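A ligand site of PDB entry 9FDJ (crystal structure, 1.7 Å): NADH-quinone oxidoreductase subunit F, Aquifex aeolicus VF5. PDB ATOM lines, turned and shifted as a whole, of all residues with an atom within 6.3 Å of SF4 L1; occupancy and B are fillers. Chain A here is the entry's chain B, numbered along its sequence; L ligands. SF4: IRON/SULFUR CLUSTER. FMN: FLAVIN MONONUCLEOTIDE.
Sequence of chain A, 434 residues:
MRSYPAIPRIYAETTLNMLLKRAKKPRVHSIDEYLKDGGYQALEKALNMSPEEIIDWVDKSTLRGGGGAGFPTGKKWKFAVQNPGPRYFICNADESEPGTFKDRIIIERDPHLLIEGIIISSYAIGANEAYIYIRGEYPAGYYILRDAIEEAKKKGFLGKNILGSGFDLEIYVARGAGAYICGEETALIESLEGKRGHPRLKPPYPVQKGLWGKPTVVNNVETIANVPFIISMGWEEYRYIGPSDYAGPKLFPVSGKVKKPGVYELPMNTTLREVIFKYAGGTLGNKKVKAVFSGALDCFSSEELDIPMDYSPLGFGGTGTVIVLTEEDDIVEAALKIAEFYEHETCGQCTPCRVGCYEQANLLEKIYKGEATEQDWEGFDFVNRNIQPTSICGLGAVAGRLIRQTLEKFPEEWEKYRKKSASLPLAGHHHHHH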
ATOM      1  N   ILE A 181      -0.812 -20.334 -20.327  1.00  0.00           N
ATOM      2  CA  ILE A 181      -1.350 -21.435 -19.539  1.00  0.00           C
ATOM      3  C   ILE A 181      -2.164 -20.930 -18.355  1.00  0.00           C
ATOM      4  O   ILE A 181      -2.986 -21.666 -17.841  1.00  0.00           O
ATOM      5  CB  ILE A 181      -0.210 -22.378 -19.108  1.00  0.00           C
ATOM      6  CG1 ILE A 181      -0.716 -23.701 -18.578  1.00  0.00           C
ATOM      7  CG2 ILE A 181       0.687 -21.660 -18.110  1.00  0.00           C
ATOM      8  CD1 ILE A 181      -1.628 -24.438 -19.519  1.00  0.00           C
ATOM      9  N   GLY A 197       1.955 -20.615 -12.758  1.00  0.00           N
ATOM     10  CA  GLY A 197       0.764 -21.098 -13.451  1.00  0.00           C
ATOM     11  C   GLY A 197       0.903 -22.560 -13.873  1.00  0.00           C
ATOM     12  O   GLY A 197       1.187 -22.868 -15.015  1.00  0.00           O
ATOM     13  N   HIS A 198       0.770 -23.447 -12.900  1.00  0.00           N
ATOM     14  CA  HIS A 198       0.902 -24.871 -13.165  1.00  0.00           C
ATOM     15  C   HIS A 198      -0.470 -25.511 -13.016  1.00  0.00           C
ATOM     16  O   HIS A 198      -1.003 -25.576 -11.907  1.00  0.00           O
ATOM     17  CB  HIS A 198       1.901 -25.502 -12.186  1.00  0.00           C
ATOM     18  CG  HIS A 198       3.336 -25.218 -12.471  1.00  0.00           C
ATOM     19  ND1 HIS A 198       4.320 -25.637 -11.603  1.00  0.00           N
ATOM     20  CD2 HIS A 198       3.979 -24.704 -13.526  1.00  0.00           C
ATOM     21  CE1 HIS A 198       5.512 -25.344 -12.106  1.00  0.00           C
ATOM     22  NE2 HIS A 198       5.325 -24.759 -13.270  1.00  0.00           N
ATOM     23  N   PRO A 199      -1.079 -26.045 -14.100  1.00  0.00           N
ATOM     24  CA  PRO A 199      -2.329 -26.792 -13.959  1.00  0.00           C
ATOM     25  C   PRO A 199      -2.273 -27.908 -12.923  1.00  0.00           C
ATOM     26  O   PRO A 199      -1.229 -28.503 -12.676  1.00  0.00           O
ATOM     27  CB  PRO A 199      -2.597 -27.309 -15.367  1.00  0.00           C
ATOM     28  CG  PRO A 199      -1.890 -26.313 -16.253  1.00  0.00           C
ATOM     29  CD  PRO A 199      -0.640 -25.902 -15.498  1.00  0.00           C
ATOM     30  N   ARG A 200      -3.434 -28.163 -12.326  1.00  0.00           N
ATOM     31  CA  ARG A 200      -3.604 -29.222 -11.355  1.00  0.00           C
ATOM     32  C   ARG A 200      -4.349 -30.364 -12.046  1.00  0.00           C
ATOM     33  O   ARG A 200      -5.161 -30.119 -12.935  1.00  0.00           O
ATOM     34  CB  ARG A 200      -4.493 -28.741 -10.192  1.00  0.00           C
ATOM     35  CG  ARG A 200      -4.025 -27.534  -9.403  1.00  0.00           C
ATOM     36  CD  ARG A 200      -5.166 -27.081  -8.443  1.00  0.00           C
ATOM     37  NE  ARG A 200      -4.835 -25.912  -7.631  1.00  0.00           N
ATOM     38  CZ  ARG A 200      -5.685 -25.332  -6.761  1.00  0.00           C
ATOM     39  NH1 ARG A 200      -6.935 -25.764  -6.657  1.00  0.00           N
ATOM     40  NH2 ARG A 200      -5.257 -24.346  -5.989  1.00  0.00           N
ATOM     41  N   GLU A 345       4.500 -21.939 -24.804  1.00  0.00           N
ATOM     42  CA  GLU A 345       3.470 -21.868 -23.773  1.00  0.00           C
ATOM     43  C   GLU A 345       3.363 -23.110 -22.883  1.00  0.00           C
ATOM     44  O   GLU A 345       2.737 -23.048 -21.829  1.00  0.00           O
ATOM     45  CB  GLU A 345       2.126 -21.450 -24.362  1.00  0.00           C
ATOM     46  CG  GLU A 345       2.147 -20.078 -25.025  1.00  0.00           C
ATOM     47  CD  GLU A 345       2.625 -18.905 -24.164  1.00  0.00           C
ATOM     48  OE1 GLU A 345       2.575 -19.018 -22.910  1.00  0.00           O
ATOM     49  OE2 GLU A 345       3.074 -17.877 -24.773  1.00  0.00           O
ATOM     50  N   THR A 346       3.956 -24.246 -23.264  1.00  0.00           N
ATOM     51  CA  THR A 346       3.935 -25.399 -22.376  1.00  0.00           C
ATOM     52  C   THR A 346       4.532 -25.003 -21.036  1.00  0.00           C
ATOM     53  O   THR A 346       5.589 -24.363 -20.988  1.00  0.00           O
ATOM     54  CB  THR A 346       4.639 -26.622 -22.972  1.00  0.00           C
ATOM     55  OG1 THR A 346       4.688 -27.611 -21.929  1.00  0.00           O
ATOM     56  CG2 THR A 346       6.060 -26.362 -23.450  1.00  0.00           C
ATOM     57  N   CYS A 347       3.877 -25.401 -19.923  1.00  0.00           N
ATOM     58  CA  CYS A 347       4.393 -25.079 -18.600  1.00  0.00           C
ATOM     59  C   CYS A 347       5.526 -26.028 -18.171  1.00  0.00           C
ATOM     60  O   CYS A 347       6.232 -25.752 -17.196  1.00  0.00           O
ATOM     61  CB  CYS A 347       3.267 -25.006 -17.563  1.00  0.00           C
ATOM     62  SG  CYS A 347       2.744 -26.616 -16.906  1.00  0.00           S
ATOM     63  N   GLY A 348       5.675 -27.167 -18.865  1.00  0.00           N
ATOM     64  CA  GLY A 348       6.789 -28.076 -18.645  1.00  0.00           C
ATOM     65  C   GLY A 348       6.578 -29.138 -17.551  1.00  0.00           C
ATOM     66  O   GLY A 348       7.497 -29.924 -17.299  1.00  0.00           O
ATOM     67  N   GLN A 349       5.401 -29.198 -16.911  1.00  0.00           N
ATOM     68  CA  GLN A 349       5.170 -30.167 -15.835  1.00  0.00           C
ATOM     69  C   GLN A 349       5.165 -31.618 -16.325  1.00  0.00           C
ATOM     70  O   GLN A 349       5.581 -32.546 -15.595  1.00  0.00           O
ATOM     71  CB  GLN A 349       3.802 -29.983 -15.174  1.00  0.00           C
ATOM     72  CG  GLN A 349       3.688 -28.825 -14.199  1.00  0.00           C
ATOM     73  CD  GLN A 349       2.340 -28.876 -13.500  1.00  0.00           C
ATOM     74  OE1 GLN A 349       1.293 -28.489 -14.045  1.00  0.00           O
ATOM     75  NE2 GLN A 349       2.361 -29.423 -12.293  1.00  0.00           N
ATOM     76  N   CYS A 350       4.628 -31.821 -17.530  1.00  0.00           N
ATOM     77  CA  CYS A 350       4.436 -33.149 -18.100  1.00  0.00           C
ATOM     78  C   CYS A 350       5.512 -33.365 -19.152  1.00  0.00           C
ATOM     79  O   CYS A 350       5.726 -32.488 -20.011  1.00  0.00           O
ATOM     80  CB  CYS A 350       3.040 -33.292 -18.727  1.00  0.00           C
ATOM     81  SG  CYS A 350       1.691 -32.620 -17.701  1.00  0.00           S
ATOM     82  N   THR A 351       6.141 -34.533 -19.141  1.00  0.00           N
ATOM     83  CA  THR A 351       7.322 -34.744 -19.978  1.00  0.00           C
ATOM     84  C   THR A 351       6.961 -34.728 -21.461  1.00  0.00           C
ATOM     85  O   THR A 351       7.620 -34.026 -22.239  1.00  0.00           O
ATOM     86  CB  THR A 351       8.100 -35.995 -19.552  1.00  0.00           C
ATOM     87  OG1 THR A 351       8.694 -35.607 -18.308  1.00  0.00           O
ATOM     88  CG2 THR A 351       9.207 -36.313 -20.541  1.00  0.00           C
ATOM     89  N   CYS A 353       4.559 -33.336 -23.122  1.00  0.00           N
ATOM     90  CA  CYS A 353       4.200 -31.982 -23.483  1.00  0.00           C
ATOM     91  C   CYS A 353       5.425 -31.080 -23.525  1.00  0.00           C
ATOM     92  O   CYS A 353       5.654 -30.391 -24.530  1.00  0.00           O
ATOM     93  CB  CYS A 353       3.182 -31.425 -22.503  1.00  0.00           C
ATOM     94  SG  CYS A 353       2.575 -29.763 -22.883  1.00  0.00           S
ATOM     95  N   ARG A 354       6.209 -31.097 -22.449  1.00  0.00           N
ATOM     96  CA  ARG A 354       7.437 -30.295 -22.353  1.00  0.00           C
ATOM     97  C   ARG A 354       8.361 -30.553 -23.541  1.00  0.00           C
ATOM     98  O   ARG A 354       8.783 -29.627 -24.228  1.00  0.00           O
ATOM     99  CB  ARG A 354       8.208 -30.624 -21.078  1.00  0.00           C
ATOM    100  CG  ARG A 354       9.463 -29.795 -20.838  1.00  0.00           C
ATOM    101  CD  ARG A 354      10.117 -30.085 -19.486  1.00  0.00           C
ATOM    102  NE  ARG A 354      10.588 -31.459 -19.378  1.00  0.00           N
ATOM    103  CZ  ARG A 354      10.053 -32.461 -18.696  1.00  0.00           C
ATOM    104  NH1 ARG A 354       8.938 -32.261 -17.967  1.00  0.00           N
ATOM    105  NH2 ARG A 354      10.657 -33.649 -18.725  1.00  0.00           N
ATOM    106  N   CYS A 357       6.334 -30.251 -27.306  1.00  0.00           N
ATOM    107  CA  CYS A 357       6.036 -28.926 -27.839  1.00  0.00           C
ATOM    108  C   CYS A 357       7.334 -28.292 -28.370  1.00  0.00           C
ATOM    109  O   CYS A 357       7.322 -27.663 -29.423  1.00  0.00           O
ATOM    110  CB  CYS A 357       5.372 -28.004 -26.830  1.00  0.00           C
ATOM    111  SG  CYS A 357       3.671 -28.467 -26.401  1.00  0.00           S
ATOM    112  N   ILE A 387       2.604 -35.776 -28.081  1.00  0.00           N
ATOM    113  CA  ILE A 387       2.647 -34.688 -27.112  1.00  0.00           C
ATOM    114  C   ILE A 387       1.655 -34.969 -25.985  1.00  0.00           C
ATOM    115  O   ILE A 387       1.924 -34.606 -24.838  1.00  0.00           O
ATOM    116  CB  ILE A 387       2.395 -33.329 -27.797  1.00  0.00           C
ATOM    117  CG1 ILE A 387       3.340 -33.144 -29.006  1.00  0.00           C
ATOM    118  CG2 ILE A 387       2.522 -32.166 -26.821  1.00  0.00           C
ATOM    119  CD1 ILE A 387       3.084 -31.904 -29.825  1.00  0.00           C
ATOM    120  N   THR A 390       0.124 -38.666 -20.936  1.00  0.00           N
ATOM    121  CA  THR A 390       0.335 -38.272 -19.543  1.00  0.00           C
ATOM    122  C   THR A 390      -0.027 -36.811 -19.273  1.00  0.00           C
ATOM    123  O   THR A 390       0.048 -36.387 -18.121  1.00  0.00           O
ATOM    124  CB  THR A 390       1.753 -38.615 -19.053  1.00  0.00           C
ATOM    125  OG1 THR A 390       2.663 -37.566 -19.415  1.00  0.00           O
ATOM    126  CG2 THR A 390       2.236 -39.954 -19.571  1.00  0.00           C
ATOM    127  N   SER A 391      -0.476 -36.030 -20.273  1.00  0.00           N
ATOM    128  CA  SER A 391      -0.778 -34.625 -20.085  1.00  0.00           C
ATOM    129  C   SER A 391      -1.881 -34.437 -19.042  1.00  0.00           C
ATOM    130  O   SER A 391      -2.823 -35.237 -18.949  1.00  0.00           O
ATOM    131  CB  SER A 391      -1.192 -33.970 -21.396  1.00  0.00           C
ATOM    132  OG  SER A 391      -2.320 -34.637 -21.942  1.00  0.00           O
ATOM    133  N   ILE A 392      -1.738 -33.429 -18.189  1.00  0.00           N
ATOM    134  CA  ILE A 392      -2.773 -33.193 -17.187  1.00  0.00           C
ATOM    135  C   ILE A 392      -3.693 -32.038 -17.565  1.00  0.00           C
ATOM    136  O   ILE A 392      -4.594 -31.722 -16.802  1.00  0.00           O
ATOM    137  CB  ILE A 392      -2.179 -33.051 -15.775  1.00  0.00           C
ATOM    138  CG1 ILE A 392      -1.285 -31.839 -15.600  1.00  0.00           C
ATOM    139  CG2 ILE A 392      -1.464 -34.326 -15.357  1.00  0.00           C
ATOM    140  CD1 ILE A 392      -0.450 -31.895 -14.327  1.00  0.00           C
ATOM    141  N   CYS A 393      -3.453 -31.348 -18.692  1.00  0.00           N
ATOM    142  CA  CYS A 393      -4.350 -30.274 -19.090  1.00  0.00           C
ATOM    143  C   CYS A 393      -4.531 -30.282 -20.611  1.00  0.00           C
ATOM    144  O   CYS A 393      -3.866 -31.025 -21.315  1.00  0.00           O
ATOM    145  CB  CYS A 393      -3.884 -28.916 -18.560  1.00  0.00           C
ATOM    146  SG  CYS A 393      -2.798 -27.978 -19.683  1.00  0.00           S
ATOM    147  N   GLY A 394      -5.432 -29.437 -21.102  1.00  0.00           N
ATOM    148  CA  GLY A 394      -5.789 -29.448 -22.514  1.00  0.00           C
ATOM    149  C   GLY A 394      -4.678 -29.022 -23.474  1.00  0.00           C
ATOM    150  O   GLY A 394      -4.736 -29.359 -24.646  1.00  0.00           O
ATOM    151  N   LEU A 395      -3.671 -28.264 -23.004  1.00  0.00           N
ATOM    152  CA  LEU A 395      -2.621 -27.789 -23.904  1.00  0.00           C
ATOM    153  C   LEU A 395      -1.900 -28.982 -24.514  1.00  0.00           C
ATOM    154  O   LEU A 395      -1.744 -29.072 -25.725  1.00  0.00           O
ATOM    155  CB  LEU A 395      -1.673 -26.838 -23.185  1.00  0.00           C
ATOM    156  CG  LEU A 395      -0.661 -26.095 -24.084  1.00  0.00           C
ATOM    157  CD1 LEU A 395      -0.191 -24.791 -23.484  1.00  0.00           C
ATOM    158  CD2 LEU A 395       0.546 -26.988 -24.356  1.00  0.00           C
ATOM    159  N   GLY A 396      -1.421 -29.908 -23.664  1.00  0.00           N
ATOM    160  CA  GLY A 396      -0.728 -31.095 -24.167  1.00  0.00           C
ATOM    161  C   GLY A 396      -1.643 -31.942 -25.055  1.00  0.00           C
ATOM    162  O   GLY A 396      -1.192 -32.499 -26.049  1.00  0.00           O
ATOM    163  N   ALA A 397      -2.925 -31.995 -24.712  1.00  0.00           N
ATOM    164  CA  ALA A 397      -3.905 -32.762 -25.445  1.00  0.00           C
ATOM    165  C   ALA A 397      -4.100 -32.238 -26.875  1.00  0.00           C
ATOM    166  O   ALA A 397      -4.403 -33.040 -27.755  1.00  0.00           O
ATOM    167  CB  ALA A 397      -5.226 -32.745 -24.691  1.00  0.00           C
HETATM  168 FE1  SF4 L   1       1.778 -27.988 -18.471  1.00  0.00          FE
HETATM  169 FE2  SF4 L   1       1.571 -29.248 -20.928  1.00  0.00          FE
HETATM  170 FE3  SF4 L   1      -0.666 -28.764 -19.455  1.00  0.00          FE
HETATM  171 FE4  SF4 L   1       1.177 -30.633 -18.632  1.00  0.00          FE
HETATM  172  S1  SF4 L   1      -0.158 -30.703 -20.544  1.00  0.00           S
HETATM  173  S2  SF4 L   1       0.134 -29.155 -17.316  1.00  0.00           S
HETATM  174  S3  SF4 L   1       3.156 -29.592 -19.326  1.00  0.00           S
HETATM  175  S4  SF4 L   1       0.804 -27.189 -20.364  1.00  0.00           S
HETATM  176  N1  FMN L   2     -10.791 -20.042 -20.737  1.00  0.00           N
HETATM  177  C2  FMN L   2     -10.985 -18.667 -20.761  1.00  0.00           C
HETATM  178  O2  FMN L   2     -12.051 -18.153 -20.337  1.00  0.00           O
HETATM  179  N3  FMN L   2      -9.964 -17.854 -21.206  1.00  0.00           N
HETATM  180  C4  FMN L   2      -8.704 -18.281 -21.625  1.00  0.00           C
HETATM  181  O4  FMN L   2      -7.851 -17.457 -21.937  1.00  0.00           O
HETATM  182  C4A FMN L   2      -8.513 -19.728 -21.586  1.00  0.00           C
HETATM  183  N5  FMN L   2      -7.326 -20.213 -21.914  1.00  0.00           N
HETATM  184  C5A FMN L   2      -7.146 -21.591 -21.758  1.00  0.00           C
HETATM  185  C6  FMN L   2      -5.877 -22.140 -22.029  1.00  0.00           C
HETATM  186  C7  FMN L   2      -5.657 -23.499 -21.913  1.00  0.00           C
HETATM  187  C7M FMN L   2      -4.283 -24.052 -22.250  1.00  0.00           C
HETATM  188  C8  FMN L   2      -6.708 -24.357 -21.542  1.00  0.00           C
HETATM  189  C8M FMN L   2      -6.553 -25.868 -21.549  1.00  0.00           C
HETATM  190  C9  FMN L   2      -7.961 -23.816 -21.247  1.00  0.00           C
HETATM  191  C9A FMN L   2      -8.184 -22.444 -21.352  1.00  0.00           C
HETATM  192  N10 FMN L   2      -9.438 -21.875 -21.056  1.00  0.00           N
HETATM  193  C10 FMN L   2      -9.608 -20.516 -21.138  1.00  0.00           C
HETATM  194  C1' FMN L   2     -10.562 -22.693 -20.607  1.00  0.00           C
HETATM  195  C2' FMN L   2     -10.696 -22.665 -19.085  1.00  0.00           C
HETATM  196  O2' FMN L   2      -9.854 -23.670 -18.487  1.00  0.00           O
HETATM  197  C3' FMN L   2     -12.149 -22.862 -18.631  1.00  0.00           C
HETATM  198  O3' FMN L   2     -12.751 -23.954 -19.312  1.00  0.00           O
HETATM  199  C4' FMN L   2     -13.055 -21.654 -18.815  1.00  0.00           C
HETATM  200  O4' FMN L   2     -12.444 -20.465 -18.290  1.00  0.00           O
HETATM  201  C5' FMN L   2     -14.371 -21.937 -18.125  1.00  0.00           C
HETATM  202  O5' FMN L   2     -15.347 -20.871 -18.359  1.00  0.00           O
HETATM  203  P   FMN L   2     -16.538 -21.122 -19.356  1.00  0.00           P
HETATM  204  O1P FMN L   2     -17.391 -19.858 -19.168  1.00  0.00           O
HETATM  205  O2P FMN L   2     -17.246 -22.387 -19.010  1.00  0.00           O
HETATM  206  O3P FMN L   2     -15.958 -21.270 -20.750  1.00  0.00           O
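Merely in contact with SF4 L1: Ile 181 (3.8 Å), Pro 199 (3.6 Å), Ser 391 (3.5 Å), Ile 392 (3.5 Å) and Leu 395 (3.8 Å).
Of the 24 residues printed, 13 come within 4 Å of SF4 L1.
The side-chain sulfur (SG) of Cys 393 lies close to the backbone NH (N) of Leu 395 (3.4 Å).
O of Gly 348 is in hydrogen-bond range of NH1 of Arg 354, 2.8 Å away.
SG of Cys 353 sits close to OG1 of Thr 346.
SG of Cys 357 sits close to O of Cys 353, at 3.3 Å.
The backbone NH of Gly 348 lies within hydrogen-bond range of the side-chain hydroxyl of Thr 346, 3.2 Å away.
OE1 of Gln 349 lies close to O of Pro 199 (2.9 Å).
The side-chain sulfur (SG) of Cys 347 sits close to the backbone NH (N) of Gln 349 (3.7 Å).
SG of Cys 350 lies close to N of Ile 392, at 3.6 Å.
A sulfur (S3) of SF4 L1 lies close to the backbone NH (N) of Gly 348.
The backbone NH of Cys 350 sits close to a sulfur (S3) of SF4 L1.
SG of Cys 353 binds FE2 of SF4 L1, 2.3 Å away.
S3 of SF4 L1 sits close to OG1 of Thr 346 (3.6 Å).
The side-chain sulfur (SG) of Cys 347 binds an iron atom (FE1) of SF4 L1 (2.3 Å).
SG of Cys 393 binds FE3 of SF4 L1.
S3 of SF4 L1 lies close to N of Gln 349.
A sulfur (S4) of SF4 L1 sits close to the backbone NH (N) of Cys 347, at 3.6 Å.
The backbone NH (N) of Gly 396 lies close to a sulfur (S1) of SF4 L1, 3.5 Å away.
An iron atom (FE4) of SF4 L1 is bound by the side-chain sulfur (SG) of Cys 350, 2.3 Å away.
OE1 of Gln 349 sits close to S2 of SF4 L1 (3.5 Å).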
